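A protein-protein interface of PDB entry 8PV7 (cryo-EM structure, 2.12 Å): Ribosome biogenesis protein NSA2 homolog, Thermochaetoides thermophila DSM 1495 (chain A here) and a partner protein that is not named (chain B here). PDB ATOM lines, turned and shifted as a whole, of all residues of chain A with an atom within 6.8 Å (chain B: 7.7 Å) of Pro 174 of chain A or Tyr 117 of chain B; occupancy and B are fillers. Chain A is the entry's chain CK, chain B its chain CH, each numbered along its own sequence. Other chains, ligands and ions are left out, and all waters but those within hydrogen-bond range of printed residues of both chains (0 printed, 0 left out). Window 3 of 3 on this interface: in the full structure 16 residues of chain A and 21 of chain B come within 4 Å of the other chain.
Pro 174 of chain A touches just one residue of chain B: Tyr 117. Printed residues of chain B within 4 Å of Gly 176 of chain A: Arg 113 (3.7 Å) and Leu 114 (3.5 Å). Of the printed residues of chain A, Arg 113 of chain B touches Gly 176. Tyr 117 of chain B touches just these residues of chain A: Pro 174 and Leu 177. Of the printed residues of chain A, Gln 119 of chain B touches Thr 152 (3.9 Å). The nearest printed residue of chain A that does not touch Tyr 117 of chain B is Ile 150 of chain A (4.4 Å). The nearest printed residue of chain B that does not touch Thr 152 of chain A is Gln 123 of chain B (4.5 Å).
Hydrophobic or aromatic side chains of chain A within 4 Å of the printed part of chain B: Pro 174 and Leu 177. Along chain A the printed residues that touch a printed residue of chain B span positions 152 to 177. Of the 15 printed residues of chain B, 4 touch a printed residue of chain A. Printed residues of chain B that touch a printed residue of chain A: Arg 113, Leu 114, Tyr 117 and Gln 119. Among the printed residues, 6 pairs touch across the chains.
N of Thr 155 of chain A lies within hydrogen-bond range of O of Leu 177 of chain A, at 3.1 Å. NH2 of Arg 42 of chain B lies close to NE2 of Gln 119 of chain B (3.4 Å). NE2 of Gln 119 of chain B sits at hydrogen-bond distance from O of Tyr 117 of chain B, 3.2 Å away. N of Gln 119 of chain B sits at hydrogen-bond distance from OE1 of Gln 123 of chain B (2.8 Å).
CG of Gln 119 of chain B touches CG2 of Thr 152 of chain A, at 3.9 Å. CB of Pro 174 of chain A touches CZ of Tyr 117 of chain B, 3.5 Å away. Arg 113 of chain B touches Gly 176 of chain A (CD to CA, 3.7 Å). CD2 of Leu 114 of chain B touches O of Gly 176 of chain A, at 3.5 Å. CD2 of Leu 114 of chain B touches CD2 of Leu 177 of chain A, 3.8 Å away. Tyr 117 of chain B touches Leu 177 of chain A.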
ATOM      1  N   ILE A 150       2.391  22.301 -25.099  1.00  0.00           N
ATOM      2  CA  ILE A 150       3.713  22.808 -24.743  1.00  0.00           C
ATOM      3  C   ILE A 150       4.414  23.289 -26.007  1.00  0.00           C
ATOM      4  O   ILE A 150       4.389  22.613 -27.043  1.00  0.00           O
ATOM      5  CB  ILE A 150       4.538  21.741 -23.993  1.00  0.00           C
ATOM      6  CG1 ILE A 150       5.948  22.246 -23.677  1.00  0.00           C
ATOM      7  CG2 ILE A 150       4.582  20.425 -24.748  1.00  0.00           C
ATOM      8  CD1 ILE A 150       6.712  21.344 -22.745  1.00  0.00           C
ATOM      9  N   VAL A 151       5.009  24.475 -25.938  1.00  0.00           N
ATOM     10  CA  VAL A 151       5.707  25.064 -27.077  1.00  0.00           C
ATOM     11  C   VAL A 151       7.113  24.479 -27.144  1.00  0.00           C
ATOM     12  O   VAL A 151       7.882  24.576 -26.183  1.00  0.00           O
ATOM     13  CB  VAL A 151       5.747  26.594 -26.965  1.00  0.00           C
ATOM     14  CG1 VAL A 151       6.355  27.211 -28.213  1.00  0.00           C
ATOM     15  CG2 VAL A 151       4.357  27.138 -26.722  1.00  0.00           C
ATOM     16  N   THR A 152       7.458  23.890 -28.284  1.00  0.00           N
ATOM     17  CA  THR A 152       8.703  23.151 -28.442  1.00  0.00           C
ATOM     18  C   THR A 152       9.848  23.985 -29.008  1.00  0.00           C
ATOM     19  O   THR A 152      10.931  23.441 -29.230  1.00  0.00           O
ATOM     20  CB  THR A 152       8.479  21.930 -29.340  1.00  0.00           C
ATOM     21  OG1 THR A 152       8.166  22.363 -30.668  1.00  0.00           O
ATOM     22  CG2 THR A 152       7.347  21.074 -28.814  1.00  0.00           C
ATOM     23  N   LYS A 153       9.651  25.274 -29.231  1.00  0.00           N
ATOM     24  CA  LYS A 153      10.661  26.149 -29.801  1.00  0.00           C
ATOM     25  C   LYS A 153      10.994  27.258 -28.809  1.00  0.00           C
ATOM     26  O   LYS A 153      10.216  27.518 -27.885  1.00  0.00           O
ATOM     27  CB  LYS A 153      10.172  26.748 -31.130  1.00  0.00           C
ATOM     28  CG  LYS A 153       9.638  25.731 -32.117  1.00  0.00           C
ATOM     29  CD  LYS A 153      10.707  24.942 -32.816  1.00  0.00           C
ATOM     30  CE  LYS A 153      10.089  24.061 -33.884  1.00  0.00           C
ATOM     31  NZ  LYS A 153      11.106  23.272 -34.615  1.00  0.00           N
ATOM     32  N   THR A 155      11.229  30.776 -27.006  1.00  0.00           N
ATOM     33  CA  THR A 155      10.274  31.874 -26.942  1.00  0.00           C
ATOM     34  C   THR A 155      10.880  33.064 -26.212  1.00  0.00           C
ATOM     35  O   THR A 155      11.922  32.966 -25.564  1.00  0.00           O
ATOM     36  CB  THR A 155       8.961  31.484 -26.240  1.00  0.00           C
ATOM     37  OG1 THR A 155       9.212  31.236 -24.854  1.00  0.00           O
ATOM     38  CG2 THR A 155       8.335  30.255 -26.869  1.00  0.00           C
ATOM     39  N   VAL A 157       9.332  35.950 -23.556  1.00  0.00           N
ATOM     40  CA  VAL A 157       8.142  36.210 -22.751  1.00  0.00           C
ATOM     41  C   VAL A 157       8.007  37.663 -22.326  1.00  0.00           C
ATOM     42  O   VAL A 157       6.960  38.036 -21.775  1.00  0.00           O
ATOM     43  CB  VAL A 157       8.091  35.301 -21.504  1.00  0.00           C
ATOM     44  CG1 VAL A 157       8.090  33.845 -21.918  1.00  0.00           C
ATOM     45  CG2 VAL A 157       9.246  35.610 -20.566  1.00  0.00           C
ATOM     46  N   ARG A 163       3.710  33.597 -14.863  1.00  0.00           N
ATOM     47  CA  ARG A 163       3.004  32.513 -15.520  1.00  0.00           C
ATOM     48  C   ARG A 163       1.569  32.412 -15.009  1.00  0.00           C
ATOM     49  O   ARG A 163       1.277  32.720 -13.852  1.00  0.00           O
ATOM     50  CB  ARG A 163       3.761  31.206 -15.285  1.00  0.00           C
ATOM     51  CG  ARG A 163       3.277  30.016 -16.061  1.00  0.00           C
ATOM     52  CD  ARG A 163       3.383  28.779 -15.221  1.00  0.00           C
ATOM     53  NE  ARG A 163       4.750  28.291 -15.173  1.00  0.00           N
ATOM     54  CZ  ARG A 163       5.272  27.635 -14.149  1.00  0.00           C
ATOM     55  NH1 ARG A 163       4.568  27.387 -13.059  1.00  0.00           N
ATOM     56  NH2 ARG A 163       6.529  27.213 -14.225  1.00  0.00           N
ATOM     57  N   GLU A 169      -3.677  27.370 -17.516  1.00  0.00           N
ATOM     58  CA  GLU A 169      -2.511  27.522 -18.378  1.00  0.00           C
ATOM     59  C   GLU A 169      -2.644  26.530 -19.524  1.00  0.00           C
ATOM     60  O   GLU A 169      -2.318  25.352 -19.378  1.00  0.00           O
ATOM     61  CB  GLU A 169      -1.219  27.301 -17.601  1.00  0.00           C
ATOM     62  CG  GLU A 169       0.032  27.591 -18.411  1.00  0.00           C
ATOM     63  CD  GLU A 169       1.295  27.032 -17.786  1.00  0.00           C
ATOM     64  OE1 GLU A 169       1.193  26.249 -16.823  1.00  0.00           O
ATOM     65  OE2 GLU A 169       2.393  27.373 -18.267  1.00  0.00           O
ATOM     66  N   ILE A 172       2.121  26.185 -22.531  1.00  0.00           N
ATOM     67  CA  ILE A 172       3.259  26.059 -21.637  1.00  0.00           C
ATOM     68  C   ILE A 172       4.493  26.499 -22.398  1.00  0.00           C
ATOM     69  O   ILE A 172       4.875  25.879 -23.395  1.00  0.00           O
ATOM     70  CB  ILE A 172       3.416  24.619 -21.131  1.00  0.00           C
ATOM     71  CG1 ILE A 172       2.152  24.176 -20.397  1.00  0.00           C
ATOM     72  CG2 ILE A 172       4.656  24.496 -20.253  1.00  0.00           C
ATOM     73  CD1 ILE A 172       2.075  22.699 -20.175  1.00  0.00           C
ATOM     74  N   ARG A 173       5.130  27.561 -21.925  1.00  0.00           N
ATOM     75  CA  ARG A 173       6.401  27.989 -22.492  1.00  0.00           C
ATOM     76  C   ARG A 173       7.472  27.753 -21.443  1.00  0.00           C
ATOM     77  O   ARG A 173       7.644  28.582 -20.539  1.00  0.00           O
ATOM     78  CB  ARG A 173       6.349  29.461 -22.905  1.00  0.00           C
ATOM     79  CG  ARG A 173       5.439  29.714 -24.089  1.00  0.00           C
ATOM     80  CD  ARG A 173       5.326  31.184 -24.408  1.00  0.00           C
ATOM     81  NE  ARG A 173       4.493  31.883 -23.442  1.00  0.00           N
ATOM     82  CZ  ARG A 173       4.242  33.183 -23.472  1.00  0.00           C
ATOM     83  NH1 ARG A 173       4.760  33.963 -24.404  1.00  0.00           N
ATOM     84  NH2 ARG A 173       3.459  33.715 -22.542  1.00  0.00           N
ATOM     85  N   PRO A 174       8.200  26.639 -21.510  1.00  0.00           N
ATOM     86  CA  PRO A 174       9.097  26.268 -20.407  1.00  0.00           C
ATOM     87  C   PRO A 174      10.246  27.247 -20.230  1.00  0.00           C
ATOM     88  O   PRO A 174      10.754  27.816 -21.198  1.00  0.00           O
ATOM     89  CB  PRO A 174       9.596  24.876 -20.811  1.00  0.00           C
ATOM     90  CG  PRO A 174       9.290  24.745 -22.248  1.00  0.00           C
ATOM     91  CD  PRO A 174       8.096  25.574 -22.516  1.00  0.00           C
ATOM     92  N   MET A 175      10.653  27.430 -18.969  1.00  0.00           N
ATOM     93  CA  MET A 175      11.651  28.438 -18.624  1.00  0.00           C
ATOM     94  C   MET A 175      12.998  28.151 -19.263  1.00  0.00           C
ATOM     95  O   MET A 175      13.761  29.075 -19.558  1.00  0.00           O
ATOM     96  CB  MET A 175      11.816  28.535 -17.107  1.00  0.00           C
ATOM     97  CG  MET A 175      10.538  28.512 -16.313  1.00  0.00           C
ATOM     98  SD  MET A 175      10.827  28.812 -14.561  1.00  0.00           S
ATOM     99  CE  MET A 175      10.792  27.139 -13.941  1.00  0.00           C
ATOM    100  N   GLY A 176      13.312  26.877 -19.479  1.00  0.00           N
ATOM    101  CA  GLY A 176      14.574  26.518 -20.090  1.00  0.00           C
ATOM    102  C   GLY A 176      14.680  26.867 -21.552  1.00  0.00           C
ATOM    103  O   GLY A 176      15.786  26.824 -22.099  1.00  0.00           O
ATOM    104  N   LEU A 177      13.566  27.201 -22.194  1.00  0.00           N
ATOM    105  CA  LEU A 177      13.543  27.614 -23.587  1.00  0.00           C
ATOM    106  C   LEU A 177      13.290  29.106 -23.749  1.00  0.00           C
ATOM    107  O   LEU A 177      13.144  29.581 -24.875  1.00  0.00           O
ATOM    108  CB  LEU A 177      12.491  26.807 -24.349  1.00  0.00           C
ATOM    109  CG  LEU A 177      12.903  25.400 -24.780  1.00  0.00           C
ATOM    110  CD1 LEU A 177      11.695  24.609 -25.228  1.00  0.00           C
ATOM    111  CD2 LEU A 177      13.916  25.478 -25.899  1.00  0.00           C
ATOM    112  N   ARG A 178      13.226  29.856 -22.656  1.00  0.00           N
ATOM    113  CA  ARG A 178      13.033  31.294 -22.729  1.00  0.00           C
ATOM    114  C   ARG A 178      14.372  31.986 -22.952  1.00  0.00           C
ATOM    115  O   ARG A 178      15.363  31.664 -22.293  1.00  0.00           O
ATOM    116  CB  ARG A 178      12.362  31.820 -21.463  1.00  0.00           C
ATOM    117  CG  ARG A 178      11.001  31.224 -21.185  1.00  0.00           C
ATOM    118  CD  ARG A 178      10.445  31.755 -19.884  1.00  0.00           C
ATOM    119  NE  ARG A 178       9.355  30.932 -19.381  1.00  0.00           N
ATOM    120  CZ  ARG A 178       8.780  31.090 -18.197  1.00  0.00           C
ATOM    121  NH1 ARG A 178       9.144  32.057 -17.375  1.00  0.00           N
ATOM    122  NH2 ARG A 178       7.820  30.252 -17.829  1.00  0.00           N
ATOM    123  N   ILE B  38      12.031   8.675 -27.799  1.00  0.00           N
ATOM    124  CA  ILE B  38      12.637   9.998 -27.713  1.00  0.00           C
ATOM    125  C   ILE B  38      13.352  10.188 -26.380  1.00  0.00           C
ATOM    126  O   ILE B  38      14.368  10.887 -26.314  1.00  0.00           O
ATOM    127  CB  ILE B  38      11.576  11.092 -27.981  1.00  0.00           C
ATOM    128  CG1 ILE B  38      12.216  12.480 -28.083  1.00  0.00           C
ATOM    129  CG2 ILE B  38      10.472  11.079 -26.946  1.00  0.00           C
ATOM    130  CD1 ILE B  38      13.253  12.602 -29.177  1.00  0.00           C
ATOM    131  N   ARG B  42      17.216  11.271 -26.074  1.00  0.00           N
ATOM    132  CA  ARG B  42      17.608  12.361 -25.188  1.00  0.00           C
ATOM    133  C   ARG B  42      18.659  11.911 -24.189  1.00  0.00           C
ATOM    134  O   ARG B  42      19.623  12.638 -23.935  1.00  0.00           O
ATOM    135  CB  ARG B  42      16.392  12.902 -24.443  1.00  0.00           C
ATOM    136  CG  ARG B  42      15.475  13.784 -25.246  1.00  0.00           C
ATOM    137  CD  ARG B  42      14.222  14.043 -24.447  1.00  0.00           C
ATOM    138  NE  ARG B  42      13.198  14.730 -25.217  1.00  0.00           N
ATOM    139  CZ  ARG B  42      11.920  14.770 -24.875  1.00  0.00           C
ATOM    140  NH1 ARG B  42      11.474  14.138 -23.804  1.00  0.00           N
ATOM    141  NH2 ARG B  42      11.068  15.451 -25.632  1.00  0.00           N
ATOM    142  N   TYR B 111      22.949  23.170 -22.434  1.00  0.00           N
ATOM    143  CA  TYR B 111      22.560  22.245 -23.490  1.00  0.00           C
ATOM    144  C   TYR B 111      21.899  20.986 -22.943  1.00  0.00           C
ATOM    145  O   TYR B 111      21.074  20.387 -23.635  1.00  0.00           O
ATOM    146  CB  TYR B 111      23.766  21.916 -24.362  1.00  0.00           C
ATOM    147  CG  TYR B 111      24.017  23.000 -25.386  1.00  0.00           C
ATOM    148  CD1 TYR B 111      23.401  22.972 -26.627  1.00  0.00           C
ATOM    149  CD2 TYR B 111      24.836  24.075 -25.089  1.00  0.00           C
ATOM    150  CE1 TYR B 111      23.619  23.971 -27.548  1.00  0.00           C
ATOM    151  CE2 TYR B 111      25.058  25.075 -25.999  1.00  0.00           C
ATOM    152  CZ  TYR B 111      24.447  25.021 -27.229  1.00  0.00           C
ATOM    153  OH  TYR B 111      24.673  26.023 -28.136  1.00  0.00           O
ATOM    154  N   VAL B 112      22.211  20.582 -21.709  1.00  0.00           N
ATOM    155  CA  VAL B 112      21.455  19.502 -21.079  1.00  0.00           C
ATOM    156  C   VAL B 112      20.012  19.935 -20.834  1.00  0.00           C
ATOM    157  O   VAL B 112      19.060  19.174 -21.088  1.00  0.00           O
ATOM    158  CB  VAL B 112      22.159  19.055 -19.783  1.00  0.00           C
ATOM    159  CG1 VAL B 112      21.210  18.308 -18.867  1.00  0.00           C
ATOM    160  CG2 VAL B 112      23.355  18.195 -20.119  1.00  0.00           C
ATOM    161  N   ARG B 113      19.825  21.182 -20.391  1.00  0.00           N
ATOM    162  CA  ARG B 113      18.478  21.710 -20.214  1.00  0.00           C
ATOM    163  C   ARG B 113      17.708  21.759 -21.537  1.00  0.00           C
ATOM    164  O   ARG B 113      16.512  21.456 -21.568  1.00  0.00           O
ATOM    165  CB  ARG B 113      18.544  23.090 -19.565  1.00  0.00           C
ATOM    166  CG  ARG B 113      17.228  23.561 -18.993  1.00  0.00           C
ATOM    167  CD  ARG B 113      17.344  24.902 -18.298  1.00  0.00           C
ATOM    168  NE  ARG B 113      18.350  24.907 -17.245  1.00  0.00           N
ATOM    169  CZ  ARG B 113      19.483  25.591 -17.299  1.00  0.00           C
ATOM    170  NH1 ARG B 113      19.786  26.344 -18.343  1.00  0.00           N
ATOM    171  NH2 ARG B 113      20.333  25.520 -16.281  1.00  0.00           N
ATOM    172  N   LEU B 114      18.376  22.117 -22.640  1.00  0.00           N
ATOM    173  CA  LEU B 114      17.693  22.128 -23.941  1.00  0.00           C
ATOM    174  C   LEU B 114      17.385  20.714 -24.433  1.00  0.00           C
ATOM    175  O   LEU B 114      16.327  20.464 -25.037  1.00  0.00           O
ATOM    176  CB  LEU B 114      18.532  22.877 -24.974  1.00  0.00           C
ATOM    177  CG  LEU B 114      18.766  24.362 -24.710  1.00  0.00           C
ATOM    178  CD1 LEU B 114      19.666  24.956 -25.769  1.00  0.00           C
ATOM    179  CD2 LEU B 114      17.462  25.120 -24.616  1.00  0.00           C
ATOM    180  N   LEU B 115      18.296  19.772 -24.181  1.00  0.00           N
ATOM    181  CA  LEU B 115      18.069  18.391 -24.579  1.00  0.00           C
ATOM    182  C   LEU B 115      16.914  17.765 -23.818  1.00  0.00           C
ATOM    183  O   LEU B 115      16.331  16.786 -24.287  1.00  0.00           O
ATOM    184  CB  LEU B 115      19.339  17.571 -24.376  1.00  0.00           C
ATOM    185  CG  LEU B 115      20.329  17.648 -25.533  1.00  0.00           C
ATOM    186  CD1 LEU B 115      21.607  16.922 -25.193  1.00  0.00           C
ATOM    187  CD2 LEU B 115      19.701  17.072 -26.778  1.00  0.00           C
ATOM    188  N   LYS B 116      16.578  18.300 -22.639  1.00  0.00           N
ATOM    189  CA  LYS B 116      15.347  17.867 -21.976  1.00  0.00           C
ATOM    190  C   LYS B 116      14.095  18.132 -22.806  1.00  0.00           C
ATOM    191  O   LYS B 116      13.099  17.422 -22.640  1.00  0.00           O
ATOM    192  CB  LYS B 116      15.161  18.547 -20.621  1.00  0.00           C
ATOM    193  CG  LYS B 116      16.187  18.217 -19.571  1.00  0.00           C
ATOM    194  CD  LYS B 116      15.698  18.620 -18.187  1.00  0.00           C
ATOM    195  CE  LYS B 116      15.094  20.014 -18.167  1.00  0.00           C
ATOM    196  NZ  LYS B 116      14.416  20.273 -16.877  1.00  0.00           N
ATOM    197  N   TYR B 117      14.106  19.141 -23.671  1.00  0.00           N
ATOM    198  CA  TYR B 117      12.926  19.511 -24.435  1.00  0.00           C
ATOM    199  C   TYR B 117      13.025  19.176 -25.916  1.00  0.00           C
ATOM    200  O   TYR B 117      12.033  19.343 -26.629  1.00  0.00           O
ATOM    201  CB  TYR B 117      12.638  21.006 -24.261  1.00  0.00           C
ATOM    202  CG  TYR B 117      12.296  21.396 -22.844  1.00  0.00           C
ATOM    203  CD1 TYR B 117      11.088  21.026 -22.277  1.00  0.00           C
ATOM    204  CD2 TYR B 117      13.186  22.124 -22.070  1.00  0.00           C
ATOM    205  CE1 TYR B 117      10.775  21.372 -20.984  1.00  0.00           C
ATOM    206  CE2 TYR B 117      12.880  22.480 -20.776  1.00  0.00           C
ATOM    207  CZ  TYR B 117      11.674  22.100 -20.237  1.00  0.00           C
ATOM    208  OH  TYR B 117      11.364  22.450 -18.949  1.00  0.00           O
ATOM    209  N   ALA B 118      14.185  18.727 -26.401  1.00  0.00           N
ATOM    210  CA  ALA B 118      14.315  18.381 -27.817  1.00  0.00           C
ATOM    211  C   ALA B 118      13.375  17.238 -28.219  1.00  0.00           C
ATOM    212  O   ALA B 118      13.110  16.317 -27.446  1.00  0.00           O
ATOM    213  CB  ALA B 118      15.754  18.004 -28.146  1.00  0.00           C
ATOM    214  N   GLN B 119      12.864  17.311 -29.450  1.00  0.00           N
ATOM    215  CA  GLN B 119      11.741  16.484 -29.880  1.00  0.00           C
ATOM    216  C   GLN B 119      12.083  15.464 -30.959  1.00  0.00           C
ATOM    217  O   GLN B 119      11.198  14.709 -31.368  1.00  0.00           O
ATOM    218  CB  GLN B 119      10.596  17.372 -30.386  1.00  0.00           C
ATOM    219  CG  GLN B 119       9.957  18.229 -29.315  1.00  0.00           C
ATOM    220  CD  GLN B 119       9.177  17.416 -28.314  1.00  0.00           C
ATOM    221  OE1 GLN B 119       8.576  16.405 -28.656  1.00  0.00           O
ATOM    222  NE2 GLN B 119       9.189  17.851 -27.064  1.00  0.00           N
ATOM    223  N   SER B 120      13.320  15.419 -31.441  1.00  0.00           N
ATOM    224  CA  SER B 120      13.674  14.475 -32.491  1.00  0.00           C
ATOM    225  C   SER B 120      15.160  14.170 -32.416  1.00  0.00           C
ATOM    226  O   SER B 120      15.930  14.882 -31.763  1.00  0.00           O
ATOM    227  CB  SER B 120      13.303  15.007 -33.882  1.00  0.00           C
ATOM    228  OG  SER B 120      14.097  16.118 -34.246  1.00  0.00           O
ATOM    229  N   GLN B 123      17.247  17.073 -33.990  1.00  0.00           N
ATOM    230  CA  GLN B 123      17.404  18.207 -33.084  1.00  0.00           C
ATOM    231  C   GLN B 123      18.363  17.876 -31.946  1.00  0.00           C
ATOM    232  O   GLN B 123      19.211  18.698 -31.575  1.00  0.00           O
ATOM    233  CB  GLN B 123      16.042  18.627 -32.537  1.00  0.00           C
ATOM    234  CG  GLN B 123      16.082  19.852 -31.652  1.00  0.00           C
ATOM    235  CD  GLN B 123      14.753  20.138 -31.002  1.00  0.00           C
ATOM    236  OE1 GLN B 123      13.812  19.363 -31.124  1.00  0.00           O
ATOM    237  NE2 GLN B 123      14.667  21.259 -30.306  1.00  0.00           N
ATOM    238  N   CYS B 124      18.247  16.664 -31.392  1.00  0.00           N
ATOM    239  CA  CYS B 124      19.160  16.222 -30.340  1.00  0.00           C
ATOM    240  C   CYS B 124      20.601  16.180 -30.832  1.00  0.00           C
ATOM    241  O   CYS B 124      21.521  16.607 -30.122  1.00  0.00           O
ATOM    242  CB  CYS B 124      18.735  14.848 -29.824  1.00  0.00           C
ATOM    243  SG  CYS B 124      17.354  14.817 -28.684  1.00  0.00           S
ATOM    244  N   LEU B 127      21.936  19.780 -31.225  1.00  0.00           N
ATOM    245  CA  LEU B 127      22.251  20.399 -29.938  1.00  0.00           C
ATOM    246  C   LEU B 127      23.516  19.805 -29.323  1.00  0.00           C
ATOM    247  O   LEU B 127      24.327  20.534 -28.735  1.00  0.00           O
ATOM    248  CB  LEU B 127      21.066  20.260 -28.987  1.00  0.00           C
ATOM    249  CG  LEU B 127      19.829  21.092 -29.327  1.00  0.00           C
ATOM    250  CD1 LEU B 127      18.653  20.662 -28.476  1.00  0.00           C
ATOM    251  CD2 LEU B 127      20.108  22.574 -29.165  1.00  0.00           C
